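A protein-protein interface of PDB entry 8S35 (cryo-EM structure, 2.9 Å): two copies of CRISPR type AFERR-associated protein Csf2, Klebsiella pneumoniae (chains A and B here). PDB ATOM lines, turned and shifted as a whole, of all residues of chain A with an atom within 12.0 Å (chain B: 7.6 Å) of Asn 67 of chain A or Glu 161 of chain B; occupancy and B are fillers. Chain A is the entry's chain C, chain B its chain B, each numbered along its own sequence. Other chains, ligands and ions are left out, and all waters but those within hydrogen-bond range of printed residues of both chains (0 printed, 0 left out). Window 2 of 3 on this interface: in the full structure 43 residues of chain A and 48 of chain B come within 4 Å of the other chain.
A ring nitrogen (NE2) of His 57 of chain A lies within hydrogen-bond range of a ring nitrogen (ND1) of His 79 of chain A (3.0 Å). OD1 of Asn 67 of chain A lies close to O of Lys 71 of chain A, 2.6 Å away. The side-chain amide oxygen (OD1) of Asn 67 of chain A sits close to the side-chain carboxylate (OD1) of Asp 69 of chain A (2.6 Å). N of Lys 71 of chain A lies within hydrogen-bond range of OD1 of Asp 69 of chain A (3.4 Å). OG of Ser 72 of chain A sits close to N of Phe 74 of chain A (3.2 Å).
Of the 23 printed residues of chain A, 10 touch a printed residue of chain B. Hydrophobic or aromatic side chains of chain A that line the printed part of chain B: Val 61, Leu 66, Leu 76, Ala 77 and His 79. Hydrophobic or aromatic side chains of chain B within 4 Å of the printed part of chain A: Phe 159, Leu 160 and Leu 168. Among the printed residues, Asp or Glu carboxylates within 4 Å of a Lys or Arg side-chain nitrogen of the other chain: Asp 75 of chain A with Arg 167 of chain B (2.9 Å).
Of chain B, only Glu 161 comes within 4 Å of Asn 67 of chain A. Printed residues of chain A within 4 Å of Glu 161 of chain B: Asn 67 (3.9 Å), Lys 71 (3.2 Å) and Ser 72 (3.6 Å). Leu 160 of chain B touches two residues of chain A. No residue of chain A comes within 4 Å of Thr 162 of chain B. Gln 164 of chain B touches just these residues of chain A: Asp 75 and Leu 76. No residue of chain A comes within 4 Å of Val 165 of chain B. Of the printed residues of chain B, Ala 77 of chain A touches Arg 167. Printed residues of chain B within 4 Å of Leu 66 of chain A: Phe 159. Ala 68 of chain A touches none of the printed residues of chain B. The nearest residue of chain A that does not touch Glu 161 of chain B is Phe 74 of chain A (5.1 Å).
No position is printed for both chains.
CG of Phe 159 of chain B touches CG1 of Val 61 of chain A, at 3.96 Å. Leu 66 of chain A touches Phe 159 of chain B (CD1 to CE1, 3.6 Å). Glu 161 of chain B touches Asn 67 of chain A. Lys 71 of chain A touches Glu 158 of chain B. Phe 159 of chain B touches Lys 71 of chain A (CA to CA, 3.99 Å). Lys 71 of chain A touches Glu 161 of chain B. O of Ser 72 of chain A touches OE1 of Glu 161 of chain B (3.6 Å). CD1 of Leu 76 of chain A touches CD1 of Leu 160 of chain B, 3.8 Å away. Leu 76 of chain A touches Leu 168 of chain B (CD1 to CB, 3.7 Å). His 79 of chain A touches Phe 159 of chain B.
The backbone NH of Leu 76 of chain A sits close to the side-chain amide oxygen of Gln 164 of chain B, 3.4 Å away. OD2 of Asp 75 of chain A is in salt-bridge range of NH1 of Arg 167 of chain B, at 2.9 Å. O of Leu 160 of chain B sits close to NZ of Lys 71 of chain A, 3.3 Å away. O of Gly 70 of chain A sits close to O of Glu 158 of chain B, at 2.6 Å. The side-chain carboxylate of Asp 75 of chain A lies close to the side-chain amide oxygen of Gln 164 of chain B, 2.6 Å away. The backbone NH (N) of Ser 72 of chain A sits at hydrogen-bond distance from the backbone carbonyl oxygen (O) of Phe 159 of chain B (3.0 Å).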
ATOM      1  N   HIS A  57     -20.460  -7.960   8.650  1.00  0.00           N
ATOM      2  CA  HIS A  57     -19.238  -8.227   7.906  1.00  0.00           C
ATOM      3  C   HIS A  57     -19.065  -9.720   7.670  1.00  0.00           C
ATOM      4  O   HIS A  57     -18.706 -10.146   6.567  1.00  0.00           O
ATOM      5  CB  HIS A  57     -18.040  -7.656   8.660  1.00  0.00           C
ATOM      6  CG  HIS A  57     -16.722  -8.123   8.134  1.00  0.00           C
ATOM      7  ND1 HIS A  57     -15.826  -8.838   8.898  1.00  0.00           N
ATOM      8  CD2 HIS A  57     -16.147  -7.977   6.917  1.00  0.00           C
ATOM      9  CE1 HIS A  57     -14.756  -9.113   8.175  1.00  0.00           C
ATOM     10  NE2 HIS A  57     -14.925  -8.601   6.969  1.00  0.00           N
ATOM     11  N   ILE A  60     -21.486 -10.825   4.992  1.00  0.00           N
ATOM     12  CA  ILE A  60     -21.014 -10.515   3.648  1.00  0.00           C
ATOM     13  C   ILE A  60     -19.876 -11.446   3.256  1.00  0.00           C
ATOM     14  O   ILE A  60     -19.767 -11.859   2.095  1.00  0.00           O
ATOM     15  CB  ILE A  60     -20.589  -9.037   3.561  1.00  0.00           C
ATOM     16  CG1 ILE A  60     -21.796  -8.106   3.745  1.00  0.00           C
ATOM     17  CG2 ILE A  60     -19.880  -8.757   2.244  1.00  0.00           C
ATOM     18  CD1 ILE A  60     -22.936  -8.312   2.760  1.00  0.00           C
ATOM     19  N   VAL A  61     -19.010 -11.787   4.210  1.00  0.00           N
ATOM     20  CA  VAL A  61     -17.914 -12.707   3.922  1.00  0.00           C
ATOM     21  C   VAL A  61     -18.466 -14.055   3.480  1.00  0.00           C
ATOM     22  O   VAL A  61     -18.001 -14.648   2.501  1.00  0.00           O
ATOM     23  CB  VAL A  61     -16.997 -12.845   5.151  1.00  0.00           C
ATOM     24  CG1 VAL A  61     -16.029 -14.010   4.977  1.00  0.00           C
ATOM     25  CG2 VAL A  61     -16.246 -11.542   5.397  1.00  0.00           C
ATOM     26  N   ASP A  62     -19.474 -14.555   4.195  1.00  0.00           N
ATOM     27  CA  ASP A  62     -20.079 -15.827   3.821  1.00  0.00           C
ATOM     28  C   ASP A  62     -20.812 -15.720   2.490  1.00  0.00           C
ATOM     29  O   ASP A  62     -20.767 -16.647   1.674  1.00  0.00           O
ATOM     30  CB  ASP A  62     -21.029 -16.297   4.920  1.00  0.00           C
ATOM     31  CG  ASP A  62     -20.297 -16.890   6.104  1.00  0.00           C
ATOM     32  OD1 ASP A  62     -19.101 -16.577   6.278  1.00  0.00           O
ATOM     33  OD2 ASP A  62     -20.914 -17.669   6.858  1.00  0.00           O
ATOM     34  N   ARG A  63     -21.495 -14.598   2.254  1.00  0.00           N
ATOM     35  CA  ARG A  63     -22.237 -14.429   1.011  1.00  0.00           C
ATOM     36  C   ARG A  63     -21.301 -14.441  -0.188  1.00  0.00           C
ATOM     37  O   ARG A  63     -21.576 -15.096  -1.200  1.00  0.00           O
ATOM     38  CB  ARG A  63     -23.035 -13.128   1.054  1.00  0.00           C
ATOM     39  CG  ARG A  63     -23.957 -12.953  -0.132  1.00  0.00           C
ATOM     40  CD  ARG A  63     -24.928 -11.807   0.066  1.00  0.00           C
ATOM     41  NE  ARG A  63     -25.980 -11.837  -0.942  1.00  0.00           N
ATOM     42  CZ  ARG A  63     -25.795 -11.579  -2.230  1.00  0.00           C
ATOM     43  NH1 ARG A  63     -24.616 -11.209  -2.705  1.00  0.00           N
ATOM     44  NH2 ARG A  63     -26.821 -11.699  -3.067  1.00  0.00           N
ATOM     45  N   VAL A  64     -20.184 -13.719  -0.093  1.00  0.00           N
ATOM     46  CA  VAL A  64     -19.196 -13.760  -1.162  1.00  0.00           C
ATOM     47  C   VAL A  64     -18.565 -15.140  -1.235  1.00  0.00           C
ATOM     48  O   VAL A  64     -18.232 -15.623  -2.323  1.00  0.00           O
ATOM     49  CB  VAL A  64     -18.142 -12.654  -0.961  1.00  0.00           C
ATOM     50  CG1 VAL A  64     -16.932 -12.885  -1.869  1.00  0.00           C
ATOM     51  CG2 VAL A  64     -18.772 -11.282  -1.207  1.00  0.00           C
ATOM     52  N   GLY A  65     -18.386 -15.794  -0.092  1.00  0.00           N
ATOM     53  CA  GLY A  65     -17.830 -17.127  -0.046  1.00  0.00           C
ATOM     54  C   GLY A  65     -16.319 -17.125   0.059  1.00  0.00           C
ATOM     55  O   GLY A  65     -15.639 -16.114  -0.134  1.00  0.00           O
ATOM     56  N   LEU A  66     -15.791 -18.303   0.374  1.00  0.00           N
ATOM     57  CA  LEU A  66     -14.368 -18.512   0.581  1.00  0.00           C
ATOM     58  C   LEU A  66     -13.854 -19.557  -0.397  1.00  0.00           C
ATOM     59  O   LEU A  66     -14.569 -20.493  -0.766  1.00  0.00           O
ATOM     60  CB  LEU A  66     -14.074 -18.964   2.018  1.00  0.00           C
ATOM     61  CG  LEU A  66     -14.841 -18.247   3.133  1.00  0.00           C
ATOM     62  CD1 LEU A  66     -14.620 -18.942   4.464  1.00  0.00           C
ATOM     63  CD2 LEU A  66     -14.426 -16.790   3.211  1.00  0.00           C
ATOM     64  N   ASN A  67     -12.604 -19.387  -0.813  1.00  0.00           N
ATOM     65  CA  ASN A  67     -11.970 -20.351  -1.699  1.00  0.00           C
ATOM     66  C   ASN A  67     -11.693 -21.644  -0.930  1.00  0.00           C
ATOM     67  O   ASN A  67     -11.991 -21.768   0.262  1.00  0.00           O
ATOM     68  CB  ASN A  67     -10.698 -19.764  -2.310  1.00  0.00           C
ATOM     69  CG  ASN A  67      -9.755 -19.203  -1.271  1.00  0.00           C
ATOM     70  OD1 ASN A  67     -10.086 -19.138  -0.089  1.00  0.00           O
ATOM     71  ND2 ASN A  67      -8.570 -18.792  -1.707  1.00  0.00           N
ATOM     72  N   ALA A  68     -11.121 -22.626  -1.634  1.00  0.00           N
ATOM     73  CA  ALA A  68     -11.019 -23.978  -1.087  1.00  0.00           C
ATOM     74  C   ALA A  68     -10.240 -24.007   0.223  1.00  0.00           C
ATOM     75  O   ALA A  68     -10.645 -24.684   1.175  1.00  0.00           O
ATOM     76  CB  ALA A  68     -10.367 -24.904  -2.113  1.00  0.00           C
ATOM     77  N   ASP A  69      -9.125 -23.279   0.300  1.00  0.00           N
ATOM     78  CA  ASP A  69      -8.378 -23.236   1.552  1.00  0.00           C
ATOM     79  C   ASP A  69      -9.099 -22.443   2.638  1.00  0.00           C
ATOM     80  O   ASP A  69      -8.656 -22.467   3.791  1.00  0.00           O
ATOM     81  CB  ASP A  69      -6.975 -22.666   1.322  1.00  0.00           C
ATOM     82  CG  ASP A  69      -6.993 -21.293   0.692  1.00  0.00           C
ATOM     83  OD1 ASP A  69      -8.093 -20.744   0.501  1.00  0.00           O
ATOM     84  OD2 ASP A  69      -5.905 -20.763   0.384  1.00  0.00           O
ATOM     85  N   GLY A  70     -10.181 -21.746   2.303  1.00  0.00           N
ATOM     86  CA  GLY A  70     -11.003 -21.074   3.287  1.00  0.00           C
ATOM     87  C   GLY A  70     -10.738 -19.600   3.498  1.00  0.00           C
ATOM     88  O   GLY A  70     -11.182 -19.059   4.516  1.00  0.00           O
ATOM     89  N   LYS A  71     -10.047 -18.934   2.579  1.00  0.00           N
ATOM     90  CA  LYS A  71      -9.766 -17.510   2.691  1.00  0.00           C
ATOM     91  C   LYS A  71     -10.809 -16.700   1.928  1.00  0.00           C
ATOM     92  O   LYS A  71     -11.467 -17.196   1.010  1.00  0.00           O
ATOM     93  CB  LYS A  71      -8.366 -17.191   2.163  1.00  0.00           C
ATOM     94  CG  LYS A  71      -7.282 -18.150   2.633  1.00  0.00           C
ATOM     95  CD  LYS A  71      -7.279 -18.305   4.146  1.00  0.00           C
ATOM     96  CE  LYS A  71      -5.997 -18.959   4.635  1.00  0.00           C
ATOM     97  NZ  LYS A  71      -5.912 -18.978   6.120  1.00  0.00           N
ATOM     98  N   SER A  72     -10.954 -15.434   2.326  1.00  0.00           N
ATOM     99  CA  SER A  72     -11.940 -14.570   1.685  1.00  0.00           C
ATOM    100  C   SER A  72     -11.299 -13.784   0.542  1.00  0.00           C
ATOM    101  O   SER A  72     -10.128 -13.402   0.636  1.00  0.00           O
ATOM    102  CB  SER A  72     -12.535 -13.590   2.688  1.00  0.00           C
ATOM    103  OG  SER A  72     -13.216 -12.543   2.023  1.00  0.00           O
ATOM    104  N   PRO A  73     -12.015 -13.519  -0.558  1.00  0.00           N
ATOM    105  CA  PRO A  73     -11.423 -12.685  -1.617  1.00  0.00           C
ATOM    106  C   PRO A  73     -11.066 -11.281  -1.161  1.00  0.00           C
ATOM    107  O   PRO A  73     -10.161 -10.666  -1.738  1.00  0.00           O
ATOM    108  CB  PRO A  73     -12.513 -12.657  -2.698  1.00  0.00           C
ATOM    109  CG  PRO A  73     -13.369 -13.827  -2.423  1.00  0.00           C
ATOM    110  CD  PRO A  73     -13.343 -14.026  -0.947  1.00  0.00           C
ATOM    111  N   PHE A  74     -11.756 -10.752  -0.153  1.00  0.00           N
ATOM    112  CA  PHE A  74     -11.542  -9.373   0.262  1.00  0.00           C
ATOM    113  C   PHE A  74     -10.111  -9.147   0.729  1.00  0.00           C
ATOM    114  O   PHE A  74      -9.512  -9.995   1.396  1.00  0.00           O
ATOM    115  CB  PHE A  74     -12.499  -9.001   1.397  1.00  0.00           C
ATOM    116  CG  PHE A  74     -13.954  -9.086   1.039  1.00  0.00           C
ATOM    117  CD1 PHE A  74     -14.402  -8.804  -0.241  1.00  0.00           C
ATOM    118  CD2 PHE A  74     -14.881  -9.439   2.002  1.00  0.00           C
ATOM    119  CE1 PHE A  74     -15.742  -8.883  -0.550  1.00  0.00           C
ATOM    120  CE2 PHE A  74     -16.219  -9.518   1.697  1.00  0.00           C
ATOM    121  CZ  PHE A  74     -16.650  -9.238   0.422  1.00  0.00           C
ATOM    122  N   ASP A  75      -9.568  -7.988   0.371  1.00  0.00           N
ATOM    123  CA  ASP A  75      -8.300  -7.552   0.923  1.00  0.00           C
ATOM    124  C   ASP A  75      -8.473  -7.212   2.400  1.00  0.00           C
ATOM    125  O   ASP A  75      -9.579  -6.948   2.877  1.00  0.00           O
ATOM    126  CB  ASP A  75      -7.775  -6.338   0.154  1.00  0.00           C
ATOM    127  CG  ASP A  75      -6.322  -6.033   0.455  1.00  0.00           C
ATOM    128  OD1 ASP A  75      -5.768  -6.629   1.401  1.00  0.00           O
ATOM    129  OD2 ASP A  75      -5.732  -5.192  -0.255  1.00  0.00           O
ATOM    130  N   LEU A  76      -7.356  -7.224   3.130  1.00  0.00           N
ATOM    131  CA  LEU A  76      -7.400  -6.860   4.542  1.00  0.00           C
ATOM    132  C   LEU A  76      -7.933  -5.445   4.721  1.00  0.00           C
ATOM    133  O   LEU A  76      -8.725  -5.176   5.635  1.00  0.00           O
ATOM    134  CB  LEU A  76      -6.011  -7.000   5.155  1.00  0.00           C
ATOM    135  CG  LEU A  76      -5.924  -6.680   6.648  1.00  0.00           C
ATOM    136  CD1 LEU A  76      -5.192  -7.781   7.386  1.00  0.00           C
ATOM    137  CD2 LEU A  76      -5.247  -5.341   6.884  1.00  0.00           C
ATOM    138  N   ALA A  77      -7.508  -4.526   3.852  1.00  0.00           N
ATOM    139  CA  ALA A  77      -8.044  -3.171   3.884  1.00  0.00           C
ATOM    140  C   ALA A  77      -9.551  -3.180   3.683  1.00  0.00           C
ATOM    141  O   ALA A  77     -10.271  -2.386   4.296  1.00  0.00           O
ATOM    142  CB  ALA A  77      -7.365  -2.312   2.819  1.00  0.00           C
ATOM    143  N   GLU A  78     -10.050  -4.076   2.829  1.00  0.00           N
ATOM    144  CA  GLU A  78     -11.491  -4.160   2.622  1.00  0.00           C
ATOM    145  C   GLU A  78     -12.192  -4.696   3.862  1.00  0.00           C
ATOM    146  O   GLU A  78     -13.284  -4.233   4.210  1.00  0.00           O
ATOM    147  CB  GLU A  78     -11.797  -5.035   1.407  1.00  0.00           C
ATOM    148  CG  GLU A  78     -11.225  -4.502   0.104  1.00  0.00           C
ATOM    149  CD  GLU A  78     -11.809  -3.158  -0.286  1.00  0.00           C
ATOM    150  OE1 GLU A  78     -12.920  -2.835   0.184  1.00  0.00           O
ATOM    151  OE2 GLU A  78     -11.159  -2.426  -1.061  1.00  0.00           O
ATOM    152  N   HIS A  79     -11.587  -5.676   4.537  1.00  0.00           N
ATOM    153  CA  HIS A  79     -12.136  -6.152   5.802  1.00  0.00           C
ATOM    154  C   HIS A  79     -12.260  -5.003   6.796  1.00  0.00           C
ATOM    155  O   HIS A  79     -13.299  -4.832   7.449  1.00  0.00           O
ATOM    156  CB  HIS A  79     -11.247  -7.257   6.378  1.00  0.00           C
ATOM    157  CG  HIS A  79     -11.479  -8.611   5.779  1.00  0.00           C
ATOM    158  ND1 HIS A  79     -12.139  -9.618   6.449  1.00  0.00           N
ATOM    159  CD2 HIS A  79     -11.115  -9.133   4.585  1.00  0.00           C
ATOM    160  CE1 HIS A  79     -12.185 -10.697   5.688  1.00  0.00           C
ATOM    161  NE2 HIS A  79     -11.572 -10.428   4.550  1.00  0.00           N
ATOM    162  N   PHE A  80     -11.198  -4.201   6.923  1.00  0.00           N
ATOM    163  CA  PHE A  80     -11.224  -3.087   7.866  1.00  0.00           C
ATOM    164  C   PHE A  80     -12.261  -2.044   7.465  1.00  0.00           C
ATOM    165  O   PHE A  80     -12.996  -1.538   8.318  1.00  0.00           O
ATOM    166  CB  PHE A  80      -9.837  -2.457   7.977  1.00  0.00           C
ATOM    167  CG  PHE A  80      -8.977  -3.082   9.035  1.00  0.00           C
ATOM    168  CD1 PHE A  80      -9.252  -2.890  10.378  1.00  0.00           C
ATOM    169  CD2 PHE A  80      -7.888  -3.858   8.687  1.00  0.00           C
ATOM    170  CE1 PHE A  80      -8.462  -3.469  11.349  1.00  0.00           C
ATOM    171  CE2 PHE A  80      -7.095  -4.435   9.656  1.00  0.00           C
ATOM    172  CZ  PHE A  80      -7.382  -4.239  10.987  1.00  0.00           C
ATOM    173  N   THR A 341     -15.564  -4.546  -2.641  1.00  0.00           N
ATOM    174  CA  THR A 341     -14.164  -4.165  -2.753  1.00  0.00           C
ATOM    175  C   THR A 341     -13.999  -2.735  -3.263  1.00  0.00           C
ATOM    176  O   THR A 341     -12.916  -2.369  -3.735  1.00  0.00           O
ATOM    177  CB  THR A 341     -13.431  -5.151  -3.670  1.00  0.00           C
ATOM    178  OG1 THR A 341     -13.814  -6.490  -3.331  1.00  0.00           O
ATOM    179  CG2 THR A 341     -11.915  -5.027  -3.529  1.00  0.00           C
ATOM    180  N   MET B 157      -9.528 -14.497  11.199  1.00  0.00           N
ATOM    181  CA  MET B 157      -8.223 -14.682  10.586  1.00  0.00           C
ATOM    182  C   MET B 157      -8.216 -15.771   9.526  1.00  0.00           C
ATOM    183  O   MET B 157      -7.345 -15.758   8.650  1.00  0.00           O
ATOM    184  CB  MET B 157      -7.188 -14.991  11.657  1.00  0.00           C
ATOM    185  CG  MET B 157      -6.730 -13.749  12.375  1.00  0.00           C
ATOM    186  SD  MET B 157      -5.220 -13.110  11.651  1.00  0.00           S
ATOM    187  CE  MET B 157      -4.066 -13.616  12.901  1.00  0.00           C
ATOM    188  N   GLU B 158      -9.161 -16.709   9.579  1.00  0.00           N
ATOM    189  CA  GLU B 158      -9.232 -17.744   8.558  1.00  0.00           C
ATOM    190  C   GLU B 158      -9.648 -17.188   7.204  1.00  0.00           C
ATOM    191  O   GLU B 158      -9.540 -17.902   6.202  1.00  0.00           O
ATOM    192  CB  GLU B 158     -10.211 -18.838   8.987  1.00  0.00           C
ATOM    193  CG  GLU B 158      -9.914 -19.428  10.353  1.00  0.00           C
ATOM    194  CD  GLU B 158     -10.778 -20.632  10.667  1.00  0.00           C
ATOM    195  OE1 GLU B 158     -12.018 -20.486  10.687  1.00  0.00           O
ATOM    196  OE2 GLU B 158     -10.217 -21.725  10.892  1.00  0.00           O
ATOM    197  N   PHE B 159     -10.101 -15.938   7.153  1.00  0.00           N
ATOM    198  CA  PHE B 159     -10.503 -15.281   5.921  1.00  0.00           C
ATOM    199  C   PHE B 159      -9.381 -14.451   5.308  1.00  0.00           C
ATOM    200  O   PHE B 159      -9.630 -13.708   4.354  1.00  0.00           O
ATOM    201  CB  PHE B 159     -11.716 -14.388   6.188  1.00  0.00           C
ATOM    202  CG  PHE B 159     -12.786 -15.053   7.003  1.00  0.00           C
ATOM    203  CD1 PHE B 159     -13.185 -16.350   6.727  1.00  0.00           C
ATOM    204  CD2 PHE B 159     -13.394 -14.380   8.048  1.00  0.00           C
ATOM    205  CE1 PHE B 159     -14.170 -16.961   7.478  1.00  0.00           C
ATOM    206  CE2 PHE B 159     -14.378 -14.986   8.801  1.00  0.00           C
ATOM    207  CZ  PHE B 159     -14.767 -16.279   8.516  1.00  0.00           C
ATOM    208  N   LEU B 160      -8.158 -14.562   5.828  1.00  0.00           N
ATOM    209  CA  LEU B 160      -7.016 -13.787   5.366  1.00  0.00           C
ATOM    210  C   LEU B 160      -5.934 -14.713   4.835  1.00  0.00           C
ATOM    211  O   LEU B 160      -5.634 -15.747   5.441  1.00  0.00           O
ATOM    212  CB  LEU B 160      -6.427 -12.938   6.493  1.00  0.00           C
ATOM    213  CG  LEU B 160      -7.321 -11.890   7.151  1.00  0.00           C
ATOM    214  CD1 LEU B 160      -6.559 -11.239   8.292  1.00  0.00           C
ATOM    215  CD2 LEU B 160      -7.785 -10.852   6.143  1.00  0.00           C
ATOM    216  N   GLU B 161      -5.350 -14.333   3.704  1.00  0.00           N
ATOM    217  CA  GLU B 161      -4.230 -15.065   3.138  1.00  0.00           C
ATOM    218  C   GLU B 161      -2.958 -14.778   3.934  1.00  0.00           C
ATOM    219  O   GLU B 161      -2.909 -13.884   4.783  1.00  0.00           O
ATOM    220  CB  GLU B 161      -4.039 -14.694   1.668  1.00  0.00           C
ATOM    221  CG  GLU B 161      -4.894 -15.498   0.707  1.00  0.00           C
ATOM    222  CD  GLU B 161      -6.341 -15.053   0.709  1.00  0.00           C
ATOM    223  OE1 GLU B 161      -6.726 -14.283   1.616  1.00  0.00           O
ATOM    224  OE2 GLU B 161      -7.095 -15.471  -0.194  1.00  0.00           O
ATOM    225  N   THR B 162      -1.916 -15.562   3.651  1.00  0.00           N
ATOM    226  CA  THR B 162      -0.635 -15.370   4.327  1.00  0.00           C
ATOM    227  C   THR B 162      -0.096 -13.967   4.088  1.00  0.00           C
ATOM    228  O   THR B 162       0.440 -13.332   5.006  1.00  0.00           O
ATOM    229  CB  THR B 162       0.371 -16.417   3.852  1.00  0.00           C
ATOM    230  OG1 THR B 162      -0.270 -17.695   3.767  1.00  0.00           O
ATOM    231  CG2 THR B 162       1.546 -16.504   4.813  1.00  0.00           C
ATOM    232  N   ASP B 163      -0.229 -13.463   2.860  1.00  0.00           N
ATOM    233  CA  ASP B 163       0.228 -12.110   2.564  1.00  0.00           C
ATOM    234  C   ASP B 163      -0.545 -11.086   3.385  1.00  0.00           C
ATOM    235  O   ASP B 163       0.035 -10.121   3.891  1.00  0.00           O
ATOM    236  CB  ASP B 163       0.094 -11.819   1.069  1.00  0.00           C
ATOM    237  CG  ASP B 163      -1.326 -11.984   0.567  1.00  0.00           C
ATOM    238  OD1 ASP B 163      -2.183 -12.436   1.352  1.00  0.00           O
ATOM    239  OD2 ASP B 163      -1.584 -11.660  -0.610  1.00  0.00           O
ATOM    240  N   GLN B 164      -1.856 -11.282   3.533  1.00  0.00           N
ATOM    241  CA  GLN B 164      -2.643 -10.358   4.338  1.00  0.00           C
ATOM    242  C   GLN B 164      -2.288 -10.466   5.814  1.00  0.00           C
ATOM    243  O   GLN B 164      -2.309  -9.459   6.526  1.00  0.00           O
ATOM    244  CB  GLN B 164      -4.135 -10.618   4.132  1.00  0.00           C
ATOM    245  CG  GLN B 164      -4.606 -10.466   2.694  1.00  0.00           C
ATOM    246  CD  GLN B 164      -4.290  -9.103   2.117  1.00  0.00           C
ATOM    247  OE1 GLN B 164      -4.141  -8.127   2.851  1.00  0.00           O
ATOM    248  NE2 GLN B 164      -4.182  -9.029   0.797  1.00  0.00           N
ATOM    249  N   VAL B 165      -1.965 -11.667   6.294  1.00  0.00           N
ATOM    250  CA  VAL B 165      -1.513 -11.811   7.675  1.00  0.00           C
ATOM    251  C   VAL B 165      -0.212 -11.046   7.883  1.00  0.00           C
ATOM    252  O   VAL B 165      -0.023 -10.366   8.900  1.00  0.00           O
ATOM    253  CB  VAL B 165      -1.360 -13.302   8.030  1.00  0.00           C
ATOM    254  CG1 VAL B 165      -0.810 -13.474   9.444  1.00  0.00           C
ATOM    255  CG2 VAL B 165      -2.696 -14.026   7.877  1.00  0.00           C
ATOM    256  N   ASP B 166       0.709 -11.153   6.923  1.00  0.00           N
ATOM    257  CA  ASP B 166       1.975 -10.434   7.029  1.00  0.00           C
ATOM    258  C   ASP B 166       1.719  -8.930   6.983  1.00  0.00           C
ATOM    259  O   ASP B 166       2.366  -8.155   7.698  1.00  0.00           O
ATOM    260  CB  ASP B 166       2.907 -10.913   5.903  1.00  0.00           C
ATOM    261  CG  ASP B 166       4.239 -10.154   5.819  1.00  0.00           C
ATOM    262  OD1 ASP B 166       4.358  -8.978   6.203  1.00  0.00           O
ATOM    263  OD2 ASP B 166       5.211 -10.775   5.341  1.00  0.00           O
ATOM    264  N   ARG B 167       0.776  -8.501   6.141  1.00  0.00           N
ATOM    265  CA  ARG B 167       0.395  -7.094   6.098  1.00  0.00           C
ATOM    266  C   ARG B 167      -0.154  -6.636   7.441  1.00  0.00           C
ATOM    267  O   ARG B 167       0.128  -5.520   7.885  1.00  0.00           O
ATOM    268  CB  ARG B 167      -0.641  -6.863   4.998  1.00  0.00           C
ATOM    269  CG  ARG B 167      -1.026  -5.405   4.803  1.00  0.00           C
ATOM    270  CD  ARG B 167      -1.975  -5.228   3.632  1.00  0.00           C
ATOM    271  NE  ARG B 167      -2.379  -3.837   3.463  1.00  0.00           N
ATOM    272  CZ  ARG B 167      -3.278  -3.411   2.585  1.00  0.00           C
ATOM    273  NH1 ARG B 167      -3.904  -4.247   1.771  1.00  0.00           N
ATOM    274  NH2 ARG B 167      -3.559  -2.114   2.524  1.00  0.00           N
ATOM    275  N   LEU B 168      -0.964  -7.473   8.088  1.00  0.00           N
ATOM    276  CA  LEU B 168      -1.479  -7.132   9.410  1.00  0.00           C
ATOM    277  C   LEU B 168      -0.346  -7.004  10.417  1.00  0.00           C
ATOM    278  O   LEU B 168      -0.360  -6.110  11.272  1.00  0.00           O
ATOM    279  CB  LEU B 168      -2.479  -8.192   9.873  1.00  0.00           C
ATOM    280  CG  LEU B 168      -3.167  -7.954  11.220  1.00  0.00           C
ATOM    281  CD1 LEU B 168      -3.930  -6.641  11.227  1.00  0.00           C
ATOM    282  CD2 LEU B 168      -4.092  -9.112  11.551  1.00  0.00           C
